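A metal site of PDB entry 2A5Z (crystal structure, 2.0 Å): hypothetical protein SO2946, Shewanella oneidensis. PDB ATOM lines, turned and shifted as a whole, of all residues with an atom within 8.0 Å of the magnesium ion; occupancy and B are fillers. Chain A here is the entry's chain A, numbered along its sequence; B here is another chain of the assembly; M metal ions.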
ATOM      1  N   TYR A  53      21.512 -16.063  12.716  1.00  0.00           N
ATOM      2  CA  TYR A  53      20.462 -16.731  11.953  1.00  0.00           C
ATOM      3  C   TYR A  53      19.405 -15.732  11.516  1.00  0.00           C
ATOM      4  O   TYR A  53      18.868 -15.000  12.349  1.00  0.00           O
ATOM      5  CB  TYR A  53      19.855 -17.940  12.716  1.00  0.00           C
ATOM      6  CG  TYR A  53      18.862 -18.665  11.836  1.00  0.00           C
ATOM      7  CD1 TYR A  53      19.239 -19.148  10.565  1.00  0.00           C
ATOM      8  CD2 TYR A  53      17.541 -18.822  12.225  1.00  0.00           C
ATOM      9  CE1 TYR A  53      18.322 -19.780   9.730  1.00  0.00           C
ATOM     10  CE2 TYR A  53      16.617 -19.460  11.407  1.00  0.00           C
ATOM     11  CZ  TYR A  53      17.006 -19.921  10.170  1.00  0.00           C
ATOM     12  OH  TYR A  53      16.078 -20.533   9.370  1.00  0.00           O
ATOM     13  N   ASP A  54      19.108 -15.723  10.215  1.00  0.00           N
ATOM     14  CA  ASP A  54      18.240 -14.740   9.565  1.00  0.00           C
ATOM     15  C   ASP A  54      16.830 -15.291   9.227  1.00  0.00           C
ATOM     16  O   ASP A  54      16.064 -14.642   8.513  1.00  0.00           O
ATOM     17  CB  ASP A  54      18.930 -14.231   8.278  1.00  0.00           C
ATOM     18  CG  ASP A  54      18.727 -12.733   8.026  1.00  0.00           C
ATOM     19  OD1 ASP A  54      17.753 -12.124   8.530  1.00  0.00           O
ATOM     20  OD2 ASP A  54      19.544 -12.151   7.283  1.00  0.00           O
ATOM     21  N   PHE A  55      16.501 -16.483   9.709  1.00  0.00           N
ATOM     22  CA  PHE A  55      15.137 -17.030   9.610  1.00  0.00           C
ATOM     23  C   PHE A  55      14.560 -17.105   8.182  1.00  0.00           C
ATOM     24  O   PHE A  55      13.444 -16.660   7.921  1.00  0.00           O
ATOM     25  CB  PHE A  55      14.180 -16.308  10.586  1.00  0.00           C
ATOM     26  CG  PHE A  55      14.562 -16.503  12.028  1.00  0.00           C
ATOM     27  CD1 PHE A  55      13.997 -17.547  12.767  1.00  0.00           C
ATOM     28  CD2 PHE A  55      15.522 -15.695  12.623  1.00  0.00           C
ATOM     29  CE1 PHE A  55      14.376 -17.770  14.089  1.00  0.00           C
ATOM     30  CE2 PHE A  55      15.913 -15.905  13.941  1.00  0.00           C
ATOM     31  CZ  PHE A  55      15.330 -16.948  14.674  1.00  0.00           C
ATOM     32  N   MET A  56      15.349 -17.682   7.266  1.00  0.00           N
ATOM     33  CA  MET A  56      14.897 -17.870   5.882  1.00  0.00           C
ATOM     34  C   MET A  56      14.564 -19.322   5.543  1.00  0.00           C
ATOM     35  O   MET A  56      14.058 -19.618   4.449  1.00  0.00           O
ATOM     36  CB  MET A  56      15.944 -17.315   4.894  1.00  0.00           C
ATOM     37  CG  MET A  56      17.123 -18.267   4.582  1.00  0.00           C
ATOM     38  SD  MET A  56      18.398 -18.310   5.864  1.00  0.00           S
ATOM     39  CE  MET A  56      19.191 -16.724   5.571  1.00  0.00           C
ATOM     40  N   ILE A  81       7.131 -18.428   6.842  1.00  0.00           N
ATOM     41  CA  ILE A  81       8.230 -17.490   6.686  1.00  0.00           C
ATOM     42  C   ILE A  81       7.826 -16.426   5.654  1.00  0.00           C
ATOM     43  O   ILE A  81       7.189 -16.735   4.631  1.00  0.00           O
ATOM     44  CB  ILE A  81       9.546 -18.212   6.272  1.00  0.00           C
ATOM     45  CG1 ILE A  81       9.974 -19.252   7.331  1.00  0.00           C
ATOM     46  CG2 ILE A  81      10.660 -17.207   5.964  1.00  0.00           C
ATOM     47  CD1 ILE A  81      10.267 -18.698   8.735  1.00  0.00           C
ATOM     48  N   LEU A  82       8.183 -15.177   5.941  1.00  0.00           N
ATOM     49  CA  LEU A  82       8.008 -14.079   4.992  1.00  0.00           C
ATOM     50  C   LEU A  82       9.174 -13.098   5.050  1.00  0.00           C
ATOM     51  O   LEU A  82      10.037 -13.193   5.945  1.00  0.00           O
ATOM     52  CB  LEU A  82       6.679 -13.347   5.260  1.00  0.00           C
ATOM     53  CG  LEU A  82       6.285 -12.951   6.685  1.00  0.00           C
ATOM     54  CD1 LEU A  82       6.900 -11.629   7.100  1.00  0.00           C
ATOM     55  CD2 LEU A  82       4.785 -12.881   6.780  1.00  0.00           C
ATOM     56  N   SER A  83       9.202 -12.179   4.088  1.00  0.00           N
ATOM     57  CA  SER A  83      10.096 -11.026   4.144  1.00  0.00           C
ATOM     58  C   SER A  83       9.270  -9.738   4.055  1.00  0.00           C
ATOM     59  O   SER A  83       8.148  -9.745   3.555  1.00  0.00           O
ATOM     60  CB  SER A  83      11.148 -11.082   3.038  1.00  0.00           C
ATOM     61  OG  SER A  83      12.053 -12.155   3.254  1.00  0.00           O
ATOM     62  N   ASN A  86      13.311  -4.524   4.141  1.00  0.00           N
ATOM     63  CA  ASN A  86      14.676  -5.043   4.250  1.00  0.00           C
ATOM     64  C   ASN A  86      14.836  -6.131   5.307  1.00  0.00           C
ATOM     65  O   ASN A  86      15.936  -6.642   5.542  1.00  0.00           O
ATOM     66  CB  ASN A  86      15.675  -3.902   4.495  1.00  0.00           C
ATOM     67  CG  ASN A  86      15.964  -3.098   3.238  1.00  0.00           C
ATOM     68  OD1 ASN A  86      16.677  -3.561   2.352  1.00  0.00           O
ATOM     69  ND2 ASN A  86      15.411  -1.903   3.166  1.00  0.00           N
ATOM     70  N   HIS A  87      13.719  -6.485   5.954  1.00  0.00           N
ATOM     71  CA  HIS A  87      13.681  -7.610   6.872  1.00  0.00           C
ATOM     72  C   HIS A  87      13.503  -8.923   6.111  1.00  0.00           C
ATOM     73  O   HIS A  87      12.400  -9.396   5.854  1.00  0.00           O
ATOM     74  CB  HIS A  87      12.586  -7.393   7.922  1.00  0.00           C
ATOM     75  CG  HIS A  87      12.834  -6.185   8.765  1.00  0.00           C
ATOM     76  ND1 HIS A  87      13.743  -6.174   9.797  1.00  0.00           N
ATOM     77  CD2 HIS A  87      12.334  -4.921   8.678  1.00  0.00           C
ATOM     78  CE1 HIS A  87      13.763  -4.969  10.346  1.00  0.00           C
ATOM     79  NE2 HIS A  87      12.926  -4.189   9.680  1.00  0.00           N
ATOM     80  N   PHE A  88      14.647  -9.484   5.739  1.00  0.00           N
ATOM     81  CA  PHE A  88      14.737 -10.675   4.903  1.00  0.00           C
ATOM     82  C   PHE A  88      14.663 -11.902   5.810  1.00  0.00           C
ATOM     83  O   PHE A  88      15.534 -12.078   6.661  1.00  0.00           O
ATOM     84  CB  PHE A  88      16.071 -10.627   4.142  1.00  0.00           C
ATOM     85  CG  PHE A  88      16.451 -11.909   3.461  1.00  0.00           C
ATOM     86  CD1 PHE A  88      15.793 -12.339   2.316  1.00  0.00           C
ATOM     87  CD2 PHE A  88      17.512 -12.659   3.942  1.00  0.00           C
ATOM     88  CE1 PHE A  88      16.157 -13.517   1.672  1.00  0.00           C
ATOM     89  CE2 PHE A  88      17.895 -13.839   3.304  1.00  0.00           C
ATOM     90  CZ  PHE A  88      17.224 -14.272   2.165  1.00  0.00           C
ATOM     91  N   GLY A  89      13.622 -12.712   5.639  1.00  0.00           N
ATOM     92  CA  GLY A  89      13.418 -13.898   6.467  1.00  0.00           C
ATOM     93  C   GLY A  89      12.859 -13.564   7.836  1.00  0.00           C
ATOM     94  O   GLY A  89      13.583 -13.168   8.751  1.00  0.00           O
ATOM     95  N   VAL A  90      11.552 -13.736   7.994  1.00  0.00           N
ATOM     96  CA  VAL A  90      10.891 -13.376   9.233  1.00  0.00           C
ATOM     97  C   VAL A  90      10.027 -14.528   9.709  1.00  0.00           C
ATOM     98  O   VAL A  90       9.275 -15.119   8.925  1.00  0.00           O
ATOM     99  CB  VAL A  90      10.047 -12.060   9.080  1.00  0.00           C
ATOM    100  CG1 VAL A  90       9.411 -11.662  10.407  1.00  0.00           C
ATOM    101  CG2 VAL A  90      10.913 -10.929   8.532  1.00  0.00           C
ATOM    102  N   GLN A  91      10.155 -14.860  10.995  1.00  0.00           N
ATOM    103  CA  GLN A  91       9.388 -15.925  11.610  1.00  0.00           C
ATOM    104  C   GLN A  91       8.292 -15.355  12.523  1.00  0.00           C
ATOM    105  O   GLN A  91       8.587 -14.974  13.664  1.00  0.00           O
ATOM    106  CB  GLN A  91      10.307 -16.884  12.397  1.00  0.00           C
ATOM    107  CG  GLN A  91       9.567 -18.025  13.131  1.00  0.00           C
ATOM    108  CD  GLN A  91       8.906 -19.023  12.179  1.00  0.00           C
ATOM    109  OE1 GLN A  91       9.557 -19.946  11.683  1.00  0.00           O
ATOM    110  NE2 GLN A  91       7.620 -18.843  11.952  1.00  0.00           N
ATOM    111  N   TYR A 123      16.622  -8.457  15.900  1.00  0.00           N
ATOM    112  CA  TYR A 123      15.702  -7.644  15.114  1.00  0.00           C
ATOM    113  C   TYR A 123      14.336  -8.301  15.213  1.00  0.00           C
ATOM    114  O   TYR A 123      14.183  -9.451  14.820  1.00  0.00           O
ATOM    115  CB  TYR A 123      16.168  -7.576  13.644  1.00  0.00           C
ATOM    116  CG  TYR A 123      17.505  -6.880  13.480  1.00  0.00           C
ATOM    117  CD1 TYR A 123      17.579  -5.611  12.894  1.00  0.00           C
ATOM    118  CD2 TYR A 123      18.687  -7.470  13.920  1.00  0.00           C
ATOM    119  CE1 TYR A 123      18.800  -4.956  12.752  1.00  0.00           C
ATOM    120  CE2 TYR A 123      19.915  -6.827  13.788  1.00  0.00           C
ATOM    121  CZ  TYR A 123      19.957  -5.569  13.199  1.00  0.00           C
ATOM    122  OH  TYR A 123      21.179  -4.932  13.052  1.00  0.00           O
ATOM    123  N   TRP A 184       8.939  -2.613  13.848  1.00  0.00           N
ATOM    124  CA  TRP A 184      10.262  -3.213  13.906  1.00  0.00           C
ATOM    125  C   TRP A 184      11.178  -2.526  14.912  1.00  0.00           C
ATOM    126  O   TRP A 184      11.355  -1.304  14.882  1.00  0.00           O
ATOM    127  CB  TRP A 184      10.905  -3.228  12.520  1.00  0.00           C
ATOM    128  CG  TRP A 184      10.332  -4.286  11.637  1.00  0.00           C
ATOM    129  CD1 TRP A 184       9.429  -4.116  10.628  1.00  0.00           C
ATOM    130  CD2 TRP A 184      10.611  -5.691  11.689  1.00  0.00           C
ATOM    131  NE1 TRP A 184       9.135  -5.328  10.043  1.00  0.00           N
ATOM    132  CE2 TRP A 184       9.849  -6.311  10.681  1.00  0.00           C
ATOM    133  CE3 TRP A 184      11.454  -6.478  12.489  1.00  0.00           C
ATOM    134  CZ2 TRP A 184       9.889  -7.690  10.445  1.00  0.00           C
ATOM    135  CZ3 TRP A 184      11.490  -7.850  12.264  1.00  0.00           C
ATOM    136  CH2 TRP A 184      10.712  -8.437  11.249  1.00  0.00           C
ATOM    137  N   ILE A 246      10.408 -12.594  14.661  1.00  0.00           N
ATOM    138  CA  ILE A 246      11.851 -12.434  14.627  1.00  0.00           C
ATOM    139  C   ILE A 246      12.425 -12.495  13.214  1.00  0.00           C
ATOM    140  O   ILE A 246      12.136 -13.399  12.436  1.00  0.00           O
ATOM    141  CB  ILE A 246      12.574 -13.433  15.607  1.00  0.00           C
ATOM    142  CG1 ILE A 246      14.083 -13.140  15.660  1.00  0.00           C
ATOM    143  CG2 ILE A 246      12.255 -14.912  15.253  1.00  0.00           C
ATOM    144  CD1 ILE A 246      14.809 -13.809  16.828  1.00  0.00           C
ATOM    145  N   ASP A 247      13.245 -11.505  12.894  1.00  0.00           N
ATOM    146  CA  ASP A 247      13.933 -11.395  11.618  1.00  0.00           C
ATOM    147  C   ASP A 247      15.344 -12.006  11.726  1.00  0.00           C
ATOM    148  O   ASP A 247      15.750 -12.832  10.916  1.00  0.00           O
ATOM    149  CB  ASP A 247      13.977  -9.914  11.230  1.00  0.00           C
ATOM    150  CG  ASP A 247      14.875  -9.604  10.036  1.00  0.00           C
ATOM    151  OD1 ASP A 247      15.076 -10.458   9.164  1.00  0.00           O
ATOM    152  OD2 ASP A 247      15.345  -8.447   9.971  1.00  0.00           O
ATOM    153  N   LEU A 248      16.091 -11.604  12.762  1.00  0.00           N
ATOM    154  CA  LEU A 248      17.512 -11.879  12.788  1.00  0.00           C
ATOM    155  C   LEU A 248      18.031 -11.878  14.217  1.00  0.00           C
ATOM    156  O   LEU A 248      17.644 -11.044  15.036  1.00  0.00           O
ATOM    157  CB  LEU A 248      18.257 -10.835  11.926  1.00  0.00           C
ATOM    158  CG  LEU A 248      19.792 -10.723  11.922  1.00  0.00           C
ATOM    159  CD1 LEU A 248      20.460 -12.000  11.392  1.00  0.00           C
ATOM    160  CD2 LEU A 248      20.204  -9.506  11.113  1.00  0.00           C
ATOM    161  N   ILE A 249      18.884 -12.841  14.514  1.00  0.00           N
ATOM    162  CA  ILE A 249      19.599 -12.885  15.790  1.00  0.00           C
ATOM    163  C   ILE A 249      21.092 -13.076  15.536  1.00  0.00           C
ATOM    164  O   ILE A 249      21.497 -13.743  14.574  1.00  0.00           O
ATOM    165  CB  ILE A 249      19.001 -13.932  16.782  1.00  0.00           C
ATOM    166  CG1 ILE A 249      19.582 -13.727  18.196  1.00  0.00           C
ATOM    167  CG2 ILE A 249      19.184 -15.391  16.264  1.00  0.00           C
ATOM    168  CD1 ILE A 249      18.833 -14.455  19.296  1.00  0.00           C
ATOM    169  N   SER B  43      24.701 -16.379   5.893  1.00  0.00           N
ATOM    170  CA  SER B  43      24.086 -16.399   7.223  1.00  0.00           C
ATOM    171  C   SER B  43      23.252 -15.137   7.400  1.00  0.00           C
ATOM    172  O   SER B  43      22.032 -15.146   7.185  1.00  0.00           O
ATOM    173  CB  SER B  43      25.151 -16.539   8.322  1.00  0.00           C
ATOM    174  OG  SER B  43      26.206 -15.604   8.138  1.00  0.00           O
ATOM    175  N   ILE B  44      23.904 -14.054   7.778  1.00  0.00           N
ATOM    176  CA  ILE B  44      23.254 -12.767   7.886  1.00  0.00           C
ATOM    177  C   ILE B  44      23.390 -12.103   6.520  1.00  0.00           C
ATOM    178  O   ILE B  44      24.502 -11.882   6.041  1.00  0.00           O
ATOM    179  CB  ILE B  44      23.856 -11.932   9.067  1.00  0.00           C
ATOM    180  CG1 ILE B  44      23.348 -10.487   9.075  1.00  0.00           C
ATOM    181  CG2 ILE B  44      25.379 -11.968   9.036  1.00  0.00           C
ATOM    182  CD1 ILE B  44      23.744  -9.725  10.346  1.00  0.00           C
ATOM    183  N   ALA B  45      22.262 -11.829   5.882  1.00  0.00           N
ATOM    184  CA  ALA B  45      22.251 -11.282   4.516  1.00  0.00           C
ATOM    185  C   ALA B  45      22.419  -9.757   4.486  1.00  0.00           C
ATOM    186  O   ALA B  45      22.045  -9.052   5.426  1.00  0.00           O
ATOM    187  CB  ALA B  45      20.970 -11.689   3.804  1.00  0.00           C
ATOM    188  N   ALA B 257      18.192  -6.787   2.105  1.00  0.00           N
ATOM    189  CA  ALA B 257      18.475  -7.066   3.507  1.00  0.00           C
ATOM    190  C   ALA B 257      19.340  -5.995   4.158  1.00  0.00           C
ATOM    191  O   ALA B 257      20.059  -6.271   5.123  1.00  0.00           O
ATOM    192  CB  ALA B 257      19.118  -8.446   3.645  1.00  0.00           C
ATOM    193  N   ARG B 259      19.799  -3.448   6.601  1.00  0.00           N
ATOM    194  CA  ARG B 259      19.180  -3.028   7.853  1.00  0.00           C
ATOM    195  C   ARG B 259      20.138  -2.184   8.679  1.00  0.00           C
ATOM    196  O   ARG B 259      21.335  -2.138   8.410  1.00  0.00           O
ATOM    197  CB  ARG B 259      18.699  -4.234   8.651  1.00  0.00           C
ATOM    198  CG  ARG B 259      17.455  -4.910   8.081  1.00  0.00           C
ATOM    199  CD  ARG B 259      17.383  -6.379   8.496  1.00  0.00           C
ATOM    200  NE  ARG B 259      18.503  -7.163   7.959  1.00  0.00           N
ATOM    201  CZ  ARG B 259      18.502  -8.489   7.823  1.00  0.00           C
ATOM    202  NH1 ARG B 259      17.443  -9.198   8.162  1.00  0.00           N
ATOM    203  NH2 ARG B 259      19.571  -9.097   7.321  1.00  0.00           N
HETATM  204 MG    MG M   1      15.645 -12.530   8.778  1.00  0.00          MG
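The backbone NH of Gly 89 sits at hydrogen-bond distance from the side-chain hydroxyl of Ser 83 (2.9 Å). NH2 of Arg 259 of chain B is in salt-bridge range of OD2 of Asp 54, at 3.1 Å. The backbone NH (N) of Ala 45 of chain B sits at hydrogen-bond distance from the side-chain carboxylate (OD2) of Asp 54 (3.1 Å). The side-chain carboxylate (OD2) of Asp 247 lies within salt-bridge range of the guanidinium group (NH1) of Arg 259 of chain B (2.9 Å). The side-chain carboxylate (OD2) of Asp 247 is in hydrogen-bond range of a ring nitrogen (ND1) of His 87, 2.8 Å away. The backbone NH of Asp 247 is in hydrogen-bond range of the backbone carbonyl oxygen of Tyr 123. NH2 of Arg 259 of chain B is in hydrogen-bond range of O of Ala 45 of chain B, at 3.1 Å. NE of Arg 259 of chain B sits at hydrogen-bond distance from O of Ala 257 of chain B.
Arg 259 of chain B touches the magnesium ion (NH1 to MG, 3.8 Å). Of the 24 residues printed, 5 come within 4 Å of the magnesium ion.
The backbone carbonyl oxygen (O) of Gly 89 is bound to the magnesium ion (2.2 Å). The magnesium ion is bound by OD1 of Asp 54. The backbone carbonyl oxygen (O) of Asp 247 binds the magnesium ion. The magnesium ion is bound by O of Phe 88 (2.2 Å). The magnesium ion is bound by O of Asp 54. OD1 of Asp 247 is bound to the magnesium ion.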
